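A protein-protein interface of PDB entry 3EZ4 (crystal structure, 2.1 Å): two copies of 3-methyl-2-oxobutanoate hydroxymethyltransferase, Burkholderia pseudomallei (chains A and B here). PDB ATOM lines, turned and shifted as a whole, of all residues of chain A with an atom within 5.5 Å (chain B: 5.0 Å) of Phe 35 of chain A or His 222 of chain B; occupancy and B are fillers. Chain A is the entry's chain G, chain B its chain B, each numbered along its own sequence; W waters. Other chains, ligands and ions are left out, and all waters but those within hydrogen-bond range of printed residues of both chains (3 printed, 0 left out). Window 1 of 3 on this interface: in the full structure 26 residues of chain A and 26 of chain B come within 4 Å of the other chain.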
ATOM      1  N   SER A  30     -18.351  -7.005 -11.219  1.00  0.00           N
ATOM      2  CA  SER A  30     -19.284  -6.219 -10.441  1.00  0.00           C
ATOM      3  C   SER A  30     -20.395  -7.186 -10.007  1.00  0.00           C
ATOM      4  O   SER A  30     -20.852  -7.944 -10.833  1.00  0.00           O
ATOM      5  CB  SER A  30     -19.835  -5.128 -11.370  1.00  0.00           C
ATOM      6  OG  SER A  30     -20.635  -4.208 -10.697  1.00  0.00           O
ATOM      7  N   ASP A  32     -23.038  -6.280  -7.166  1.00  0.00           N
ATOM      8  CA  ASP A  32     -24.122  -5.686  -6.445  1.00  0.00           C
ATOM      9  C   ASP A  32     -24.403  -4.216  -6.843  1.00  0.00           C
ATOM     10  O   ASP A  32     -23.616  -3.598  -7.580  1.00  0.00           O
ATOM     11  CB  ASP A  32     -23.801  -5.803  -4.959  1.00  0.00           C
ATOM     12  CG  ASP A  32     -22.602  -4.972  -4.553  1.00  0.00           C
ATOM     13  OD1 ASP A  32     -22.763  -3.722  -4.427  1.00  0.00           O
ATOM     14  OD2 ASP A  32     -21.508  -5.549  -4.372  1.00  0.00           O
ATOM     15  N   ALA A  33     -25.499  -3.654  -6.317  1.00  0.00           N
ATOM     16  CA  ALA A  33     -25.994  -2.359  -6.779  1.00  0.00           C
ATOM     17  C   ALA A  33     -25.067  -1.182  -6.358  1.00  0.00           C
ATOM     18  O   ALA A  33     -24.878  -0.273  -7.122  1.00  0.00           O
ATOM     19  CB  ALA A  33     -27.464  -2.114  -6.293  1.00  0.00           C
ATOM     20  N   SER A  34     -24.503  -1.240  -5.162  1.00  0.00           N
ATOM     21  CA  SER A  34     -23.696  -0.162  -4.623  1.00  0.00           C
ATOM     22  C   SER A  34     -22.376  -0.050  -5.384  1.00  0.00           C
ATOM     23  O   SER A  34     -21.970   1.033  -5.790  1.00  0.00           O
ATOM     24  CB  SER A  34     -23.398  -0.402  -3.149  1.00  0.00           C
ATOM     25  OG  SER A  34     -24.527  -0.070  -2.361  1.00  0.00           O
ATOM     26  N   PHE A  35     -21.701  -1.167  -5.592  1.00  0.00           N
ATOM     27  CA  PHE A  35     -20.499  -1.100  -6.390  1.00  0.00           C
ATOM     28  C   PHE A  35     -20.825  -0.781  -7.842  1.00  0.00           C
ATOM     29  O   PHE A  35     -20.135  -0.019  -8.445  1.00  0.00           O
ATOM     30  CB  PHE A  35     -19.657  -2.341  -6.236  1.00  0.00           C
ATOM     31  CG  PHE A  35     -18.858  -2.353  -4.983  1.00  0.00           C
ATOM     32  CD1 PHE A  35     -17.691  -1.602  -4.882  1.00  0.00           C
ATOM     33  CD2 PHE A  35     -19.255  -3.116  -3.912  1.00  0.00           C
ATOM     34  CE1 PHE A  35     -16.916  -1.632  -3.725  1.00  0.00           C
ATOM     35  CE2 PHE A  35     -18.516  -3.125  -2.748  1.00  0.00           C
ATOM     36  CZ  PHE A  35     -17.320  -2.391  -2.668  1.00  0.00           C
ATOM     37  N   ALA A  36     -21.891  -1.332  -8.378  1.00  0.00           N
ATOM     38  CA  ALA A  36     -22.227  -1.047  -9.748  1.00  0.00           C
ATOM     39  C   ALA A  36     -22.393   0.462  -9.974  1.00  0.00           C
ATOM     40  O   ALA A  36     -21.970   0.998 -10.984  1.00  0.00           O
ATOM     41  CB  ALA A  36     -23.504  -1.782 -10.181  1.00  0.00           C
ATOM     42  N   ALA A  37     -23.030   1.139  -9.048  1.00  0.00           N
ATOM     43  CA  ALA A  37     -23.237   2.578  -9.181  1.00  0.00           C
ATOM     44  C   ALA A  37     -21.899   3.341  -9.001  1.00  0.00           C
ATOM     45  O   ALA A  37     -21.666   4.326  -9.668  1.00  0.00           O
ATOM     46  CB  ALA A  37     -24.288   3.068  -8.202  1.00  0.00           C
ATOM     47  N   LEU A  38     -21.056   2.897  -8.081  1.00  0.00           N
ATOM     48  CA  LEU A  38     -19.733   3.531  -7.907  1.00  0.00           C
ATOM     49  C   LEU A  38     -18.895   3.338  -9.162  1.00  0.00           C
ATOM     50  O   LEU A  38     -18.320   4.310  -9.666  1.00  0.00           O
ATOM     51  CB  LEU A  38     -19.044   3.008  -6.665  1.00  0.00           C
ATOM     52  CG  LEU A  38     -17.633   3.530  -6.361  1.00  0.00           C
ATOM     53  CD1 LEU A  38     -17.397   3.646  -4.864  1.00  0.00           C
ATOM     54  CD2 LEU A  38     -16.576   2.620  -7.045  1.00  0.00           C
ATOM     55  N   LEU A  39     -18.881   2.100  -9.710  1.00  0.00           N
ATOM     56  CA  LEU A  39     -18.137   1.834 -10.937  1.00  0.00           C
ATOM     57  C   LEU A  39     -18.592   2.699 -12.103  1.00  0.00           C
ATOM     58  O   LEU A  39     -17.738   3.207 -12.916  1.00  0.00           O
ATOM     59  CB  LEU A  39     -18.225   0.360 -11.361  1.00  0.00           C
ATOM     60  CG  LEU A  39     -17.216  -0.609 -10.739  1.00  0.00           C
ATOM     61  CD1 LEU A  39     -17.155  -0.518  -9.246  1.00  0.00           C
ATOM     62  CD2 LEU A  39     -17.509  -2.039 -11.173  1.00  0.00           C
ATOM     63  N   ASP A  40     -19.915   2.824 -12.236  1.00  0.00           N
ATOM     64  CA  ASP A  40     -20.456   3.626 -13.274  1.00  0.00           C
ATOM     65  C   ASP A  40     -20.092   5.130 -13.101  1.00  0.00           C
ATOM     66  O   ASP A  40     -19.832   5.814 -14.082  1.00  0.00           O
ATOM     67  CB  ASP A  40     -21.948   3.481 -13.381  1.00  0.00           C
ATOM     68  CG  ASP A  40     -22.434   3.810 -14.775  1.00  0.00           C
ATOM     69  OD1 ASP A  40     -21.886   3.260 -15.777  1.00  0.00           O
ATOM     70  OD2 ASP A  40     -23.385   4.582 -14.882  1.00  0.00           O
ATOM     71  N   GLN A  47     -19.224  -3.802 -17.057  1.00  0.00           N
ATOM     72  CA  GLN A  47     -19.290  -4.441 -15.755  1.00  0.00           C
ATOM     73  C   GLN A  47     -19.606  -5.884 -16.002  1.00  0.00           C
ATOM     74  O   GLN A  47     -20.553  -6.193 -16.752  1.00  0.00           O
ATOM     75  CB  GLN A  47     -20.363  -3.793 -14.890  1.00  0.00           C
ATOM     76  CG  GLN A  47     -20.020  -2.344 -14.531  1.00  0.00           C
ATOM     77  CD  GLN A  47     -20.863  -1.775 -13.436  1.00  0.00           C
ATOM     78  OE1 GLN A  47     -21.207  -2.478 -12.501  1.00  0.00           O
ATOM     79  NE2 GLN A  47     -21.129  -0.474 -13.490  1.00  0.00           N
ATOM     80  N   LEU A 221     -12.994  -7.153  -9.359  1.00  0.00           N
ATOM     81  CA  LEU A 221     -13.144  -5.991  -8.462  1.00  0.00           C
ATOM     82  C   LEU A 221     -12.418  -6.119  -7.141  1.00  0.00           C
ATOM     83  O   LEU A 221     -11.679  -5.181  -6.739  1.00  0.00           O
ATOM     84  CB  LEU A 221     -14.629  -5.727  -8.195  1.00  0.00           C
ATOM     85  CG  LEU A 221     -14.996  -4.573  -7.253  1.00  0.00           C
ATOM     86  CD1 LEU A 221     -14.533  -3.250  -7.818  1.00  0.00           C
ATOM     87  CD2 LEU A 221     -16.505  -4.534  -6.916  1.00  0.00           C
ATOM     88  N   LEU A 225      -9.024  -3.944  -5.437  1.00  0.00           N
ATOM     89  CA  LEU A 225      -9.320  -3.130  -4.237  1.00  0.00           C
ATOM     90  C   LEU A 225      -8.462  -3.581  -3.054  1.00  0.00           C
ATOM     91  O   LEU A 225      -8.548  -3.048  -1.948  1.00  0.00           O
ATOM     92  CB  LEU A 225     -10.802  -3.221  -3.867  1.00  0.00           C
ATOM     93  CG  LEU A 225     -11.704  -2.038  -4.241  1.00  0.00           C
ATOM     94  CD1 LEU A 225     -11.240  -1.234  -5.449  1.00  0.00           C
ATOM     95  CD2 LEU A 225     -13.124  -2.501  -4.378  1.00  0.00           C
ATOM     96  N   ILE A 246     -12.490   4.612  -2.186  1.00  0.00           N
ATOM     97  CA  ILE A 246     -12.751   3.489  -3.094  1.00  0.00           C
ATOM     98  C   ILE A 246     -12.999   4.023  -4.490  1.00  0.00           C
ATOM     99  O   ILE A 246     -12.474   3.496  -5.444  1.00  0.00           O
ATOM    100  CB  ILE A 246     -13.910   2.603  -2.619  1.00  0.00           C
ATOM    101  CG1 ILE A 246     -13.469   1.883  -1.339  1.00  0.00           C
ATOM    102  CG2 ILE A 246     -14.303   1.607  -3.702  1.00  0.00           C
ATOM    103  CD1 ILE A 246     -14.532   1.058  -0.630  1.00  0.00           C
ATOM    104  N   TYR B  31     -21.873  -9.509   3.959  1.00  0.00           N
ATOM    105  CA  TYR B  31     -22.749 -10.188   3.000  1.00  0.00           C
ATOM    106  C   TYR B  31     -21.965 -11.119   2.055  1.00  0.00           C
ATOM    107  O   TYR B  31     -22.580 -11.769   1.226  1.00  0.00           O
ATOM    108  CB  TYR B  31     -23.605  -9.204   2.177  1.00  0.00           C
ATOM    109  CG  TYR B  31     -24.145  -7.994   2.906  1.00  0.00           C
ATOM    110  CD1 TYR B  31     -25.249  -8.073   3.706  1.00  0.00           C
ATOM    111  CD2 TYR B  31     -23.504  -6.763   2.806  1.00  0.00           C
ATOM    112  CE1 TYR B  31     -25.739  -6.935   4.383  1.00  0.00           C
ATOM    113  CE2 TYR B  31     -23.968  -5.616   3.480  1.00  0.00           C
ATOM    114  CZ  TYR B  31     -25.084  -5.704   4.244  1.00  0.00           C
ATOM    115  OH  TYR B  31     -25.524  -4.593   4.917  1.00  0.00           O
ATOM    116  N   PHE B  35     -15.194  -9.846   2.208  1.00  0.00           N
ATOM    117  CA  PHE B  35     -15.308  -8.901   3.336  1.00  0.00           C
ATOM    118  C   PHE B  35     -15.422  -9.612   4.666  1.00  0.00           C
ATOM    119  O   PHE B  35     -14.899  -9.112   5.661  1.00  0.00           O
ATOM    120  CB  PHE B  35     -16.426  -7.893   3.134  1.00  0.00           C
ATOM    121  CG  PHE B  35     -16.112  -6.857   2.083  1.00  0.00           C
ATOM    122  CD1 PHE B  35     -15.310  -5.756   2.384  1.00  0.00           C
ATOM    123  CD2 PHE B  35     -16.603  -6.988   0.791  1.00  0.00           C
ATOM    124  CE1 PHE B  35     -14.995  -4.815   1.386  1.00  0.00           C
ATOM    125  CE2 PHE B  35     -16.322  -6.023  -0.203  1.00  0.00           C
ATOM    126  CZ  PHE B  35     -15.527  -4.955   0.092  1.00  0.00           C
ATOM    127  N   VAL B  56     -28.380  -2.083  -0.053  1.00  0.00           N
ATOM    128  CA  VAL B  56     -26.972  -1.928  -0.439  1.00  0.00           C
ATOM    129  C   VAL B  56     -26.521  -2.905  -1.534  1.00  0.00           C
ATOM    130  O   VAL B  56     -25.688  -2.520  -2.384  1.00  0.00           O
ATOM    131  CB  VAL B  56     -25.999  -1.926   0.771  1.00  0.00           C
ATOM    132  CG1 VAL B  56     -26.362  -0.733   1.704  1.00  0.00           C
ATOM    133  CG2 VAL B  56     -26.032  -3.210   1.547  1.00  0.00           C
ATOM    134  N   LEU B  57     -27.028  -4.147  -1.513  1.00  0.00           N
ATOM    135  CA  LEU B  57     -26.677  -5.125  -2.571  1.00  0.00           C
ATOM    136  C   LEU B  57     -27.680  -5.148  -3.704  1.00  0.00           C
ATOM    137  O   LEU B  57     -27.292  -5.188  -4.845  1.00  0.00           O
ATOM    138  CB  LEU B  57     -26.491  -6.553  -2.030  1.00  0.00           C
ATOM    139  CG  LEU B  57     -25.332  -6.740  -1.033  1.00  0.00           C
ATOM    140  CD1 LEU B  57     -25.196  -8.221  -0.735  1.00  0.00           C
ATOM    141  CD2 LEU B  57     -23.945  -6.170  -1.465  1.00  0.00           C
ATOM    142  N   VAL B 220     -23.807  -0.344   8.803  1.00  0.00           N
ATOM    143  CA  VAL B 220     -23.784  -0.975   7.500  1.00  0.00           C
ATOM    144  C   VAL B 220     -22.402  -0.781   6.843  1.00  0.00           C
ATOM    145  O   VAL B 220     -21.865   0.358   6.766  1.00  0.00           O
ATOM    146  CB  VAL B 220     -24.965  -0.497   6.613  1.00  0.00           C
ATOM    147  CG1 VAL B 220     -24.920  -1.153   5.240  1.00  0.00           C
ATOM    148  CG2 VAL B 220     -26.306  -0.835   7.335  1.00  0.00           C
ATOM    149  N   LEU B 221     -21.811  -1.903   6.434  1.00  0.00           N
ATOM    150  CA  LEU B 221     -20.470  -1.942   5.876  1.00  0.00           C
ATOM    151  C   LEU B 221     -20.288  -0.908   4.745  1.00  0.00           C
ATOM    152  O   LEU B 221     -19.316  -0.147   4.753  1.00  0.00           O
ATOM    153  CB  LEU B 221     -20.124  -3.344   5.373  1.00  0.00           C
ATOM    154  CG  LEU B 221     -18.774  -3.627   4.705  1.00  0.00           C
ATOM    155  CD1 LEU B 221     -17.654  -3.560   5.665  1.00  0.00           C
ATOM    156  CD2 LEU B 221     -18.765  -4.992   3.991  1.00  0.00           C
ATOM    157  N   HIS B 222     -21.219  -0.864   3.806  1.00  0.00           N
ATOM    158  CA  HIS B 222     -21.036   0.007   2.650  1.00  0.00           C
ATOM    159  C   HIS B 222     -21.070   1.487   3.042  1.00  0.00           C
ATOM    160  O   HIS B 222     -20.402   2.293   2.408  1.00  0.00           O
ATOM    161  CB  HIS B 222     -22.053  -0.332   1.562  1.00  0.00           C
ATOM    162  CG  HIS B 222     -21.876  -1.722   1.006  1.00  0.00           C
ATOM    163  ND1 HIS B 222     -22.027  -2.864   1.778  1.00  0.00           N
ATOM    164  CD2 HIS B 222     -21.504  -2.147  -0.227  1.00  0.00           C
ATOM    165  CE1 HIS B 222     -21.777  -3.928   1.031  1.00  0.00           C
ATOM    166  NE2 HIS B 222     -21.467  -3.519  -0.190  1.00  0.00           N
ATOM    167  N   ASP B 223     -21.808   1.823   4.103  1.00  0.00           N
ATOM    168  CA  ASP B 223     -21.876   3.184   4.664  1.00  0.00           C
ATOM    169  C   ASP B 223     -20.549   3.618   5.242  1.00  0.00           C
ATOM    170  O   ASP B 223     -20.042   4.692   4.952  1.00  0.00           O
ATOM    171  CB  ASP B 223     -22.960   3.265   5.770  1.00  0.00           C
ATOM    172  CG  ASP B 223     -24.380   3.294   5.210  1.00  0.00           C
ATOM    173  OD1 ASP B 223     -24.531   3.532   3.993  1.00  0.00           O
ATOM    174  OD2 ASP B 223     -25.365   3.103   5.963  1.00  0.00           O
ATOM    175  N   MET B 224     -19.965   2.747   6.043  1.00  0.00           N
ATOM    176  CA  MET B 224     -18.784   3.091   6.756  1.00  0.00           C
ATOM    177  C   MET B 224     -17.543   3.022   5.873  1.00  0.00           C
ATOM    178  O   MET B 224     -16.513   3.552   6.274  1.00  0.00           O
ATOM    179  CB  MET B 224     -18.630   2.231   8.009  1.00  0.00           C
ATOM    180  CG  MET B 224     -18.399   0.751   7.765  1.00  0.00           C
ATOM    181  SD  MET B 224     -16.682   0.243   7.678  1.00  0.00           S
ATOM    182  CE  MET B 224     -16.118   0.932   9.218  1.00  0.00           C
ATOM    183  N   LEU B 225     -17.624   2.354   4.716  1.00  0.00           N
ATOM    184  CA  LEU B 225     -16.548   2.411   3.710  1.00  0.00           C
ATOM    185  C   LEU B 225     -16.720   3.555   2.703  1.00  0.00           C
ATOM    186  O   LEU B 225     -15.925   3.720   1.777  1.00  0.00           O
ATOM    187  CB  LEU B 225     -16.487   1.118   2.918  1.00  0.00           C
ATOM    188  CG  LEU B 225     -16.081  -0.115   3.668  1.00  0.00           C
ATOM    189  CD1 LEU B 225     -16.046  -1.257   2.680  1.00  0.00           C
ATOM    190  CD2 LEU B 225     -14.725   0.123   4.410  1.00  0.00           C
ATOM    191  N   GLY B 226     -17.804   4.291   2.856  1.00  0.00           N
ATOM    192  CA  GLY B 226     -18.083   5.482   2.086  1.00  0.00           C
ATOM    193  C   GLY B 226     -18.537   5.159   0.695  1.00  0.00           C
ATOM    194  O   GLY B 226     -18.433   6.001  -0.178  1.00  0.00           O
ATOM    195  N   VAL B 227     -19.047   3.949   0.475  1.00  0.00           N
ATOM    196  CA  VAL B 227     -19.354   3.475  -0.878  1.00  0.00           C
ATOM    197  C   VAL B 227     -20.708   4.049  -1.272  1.00  0.00           C
ATOM    198  O   VAL B 227     -21.660   3.326  -1.643  1.00  0.00           O
ATOM    199  CB  VAL B 227     -19.283   1.941  -1.004  1.00  0.00           C
ATOM    200  CG1 VAL B 227     -19.876   1.495  -2.308  1.00  0.00           C
ATOM    201  CG2 VAL B 227     -17.832   1.491  -0.928  1.00  0.00           C
ATOM    202  N   PHE B 228     -20.768   5.382  -1.171  1.00  0.00           N
ATOM    203  CA  PHE B 228     -21.919   6.155  -1.580  1.00  0.00           C
ATOM    204  C   PHE B 228     -21.679   7.694  -1.578  1.00  0.00           C
ATOM    205  O   PHE B 228     -21.292   8.273  -0.542  1.00  0.00           O
ATOM    206  CB  PHE B 228     -23.144   5.819  -0.733  1.00  0.00           C
ATOM    207  CG  PHE B 228     -24.400   6.118  -1.455  1.00  0.00           C
ATOM    208  CD1 PHE B 228     -24.719   5.393  -2.593  1.00  0.00           C
ATOM    209  CD2 PHE B 228     -25.218   7.190  -1.070  1.00  0.00           C
ATOM    210  CE1 PHE B 228     -25.855   5.695  -3.310  1.00  0.00           C
ATOM    211  CE2 PHE B 228     -26.364   7.492  -1.780  1.00  0.00           C
ATOM    212  CZ  PHE B 228     -26.687   6.745  -2.900  1.00  0.00           C
HETATM  213  O   HOH W   1     -20.782  -5.528  -1.904  1.00  0.00           O
HETATM  214  O   HOH W   2     -22.439   3.589  -5.024  1.00  0.00           O
HETATM  215  O   HOH W   3     -14.506   5.281   0.014  1.00  0.00           O
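Of the 13 printed residues of chain B, 5 touch a printed residue of chain A. Hydrophobic or aromatic side chains of chain B that line the printed part of chain A: Val 56, Leu 57, His 222 and Val 227. Of the 14 printed residues of chain A, 5 touch a printed residue of chain B. Among the printed residues, no Asp or Glu carboxylate lies within 4 Å of a Lys or Arg side-chain nitrogen of the other chain.
OD1 of Asp 32 of chain A touches O of Val 56 of chain B (3.8 Å). CD2 of Leu 57 of chain B touches CB of Asp 32 of chain A, at 3.5 Å. CB of Ser 34 of chain A touches CD2 of His 222 of chain B (3.9 Å). Phe 35 of chain A touches His 222 of chain B. Leu 225 of chain B touches Ile 246 of chain A (O to CD1, 3.8 Å). CD1 of Ile 246 of chain A touches CG2 of Val 227 of chain B (3.3 Å).
The side-chain hydroxyl of Ser 34 of chain A sits at hydrogen-bond distance from the backbone carbonyl oxygen of Val 56 of chain B (2.7 Å). The backbone NH (N) of Ala 33 of chain A is in hydrogen-bond range of the backbone carbonyl oxygen (O) of Leu 57 of chain B.
Of the printed residues of chain B, Ala 33 of chain A touches Leu 57 (2.8 Å). Of the printed residues of chain B, Ser 34 of chain A touches Val 56 and His 222. Phe 35 of chain A touches just one residue of chain B: His 222. Printed residues of chain B within 4 Å of Ile 246 of chain A: Leu 225 and Val 227. Of chain A, only Ser 34 (3.9 Å) and Phe 35 (3.9 Å) come within 4 Å of His 222 of chain B. Met 224 of chain B touches none of the printed residues of chain A. Gly 226 of chain B touches none of the printed residues of chain A. Printed residues of chain A within 4 Å of Val 227 of chain B: Ile 246 (3.3 Å). The nearest residue of chain A that does not touch His 222 of chain B is Asp 32 of chain A (4.4 Å). The nearest printed residue of chain A that does not touch Val 227 of chain B is Ser 34 of chain A (4.1 Å).
O of His 222 of chain B is in hydrogen-bond range of N of Val 227 of chain B, at 2.9 Å. The side-chain carboxylate (OD1) of Asp 32 of chain A is in hydrogen-bond range of the backbone NH (N) of Phe 35 of chain A (3.0 Å). N of Ser 34 of chain A sits at hydrogen-bond distance from OD1 of Asp 32 of chain A (3.1 Å).
Water W1 lies within hydrogen-bond range of the side-chain carboxylate of Asp 32 of chain A (2.6 Å) and a ring nitrogen (NE2) of His 222 of chain B (2.7 Å). Water W2 lies within hydrogen-bond range of the backbone carbonyl oxygen (O) of Ser 34 of chain A (2.7 Å), the backbone NH (N) of Leu 38 of chain A (3.4 Å) and the backbone carbonyl oxygen (O) of Val 227 of chain B (3.5 Å). Water W3 bridges the backbone carbonyl oxygen of Leu 225 of chain B (2.7 Å) and the backbone NH of Ile 246 of chain A (3.1 Å).
Positions printed for both chains: 35, 221 and 225.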
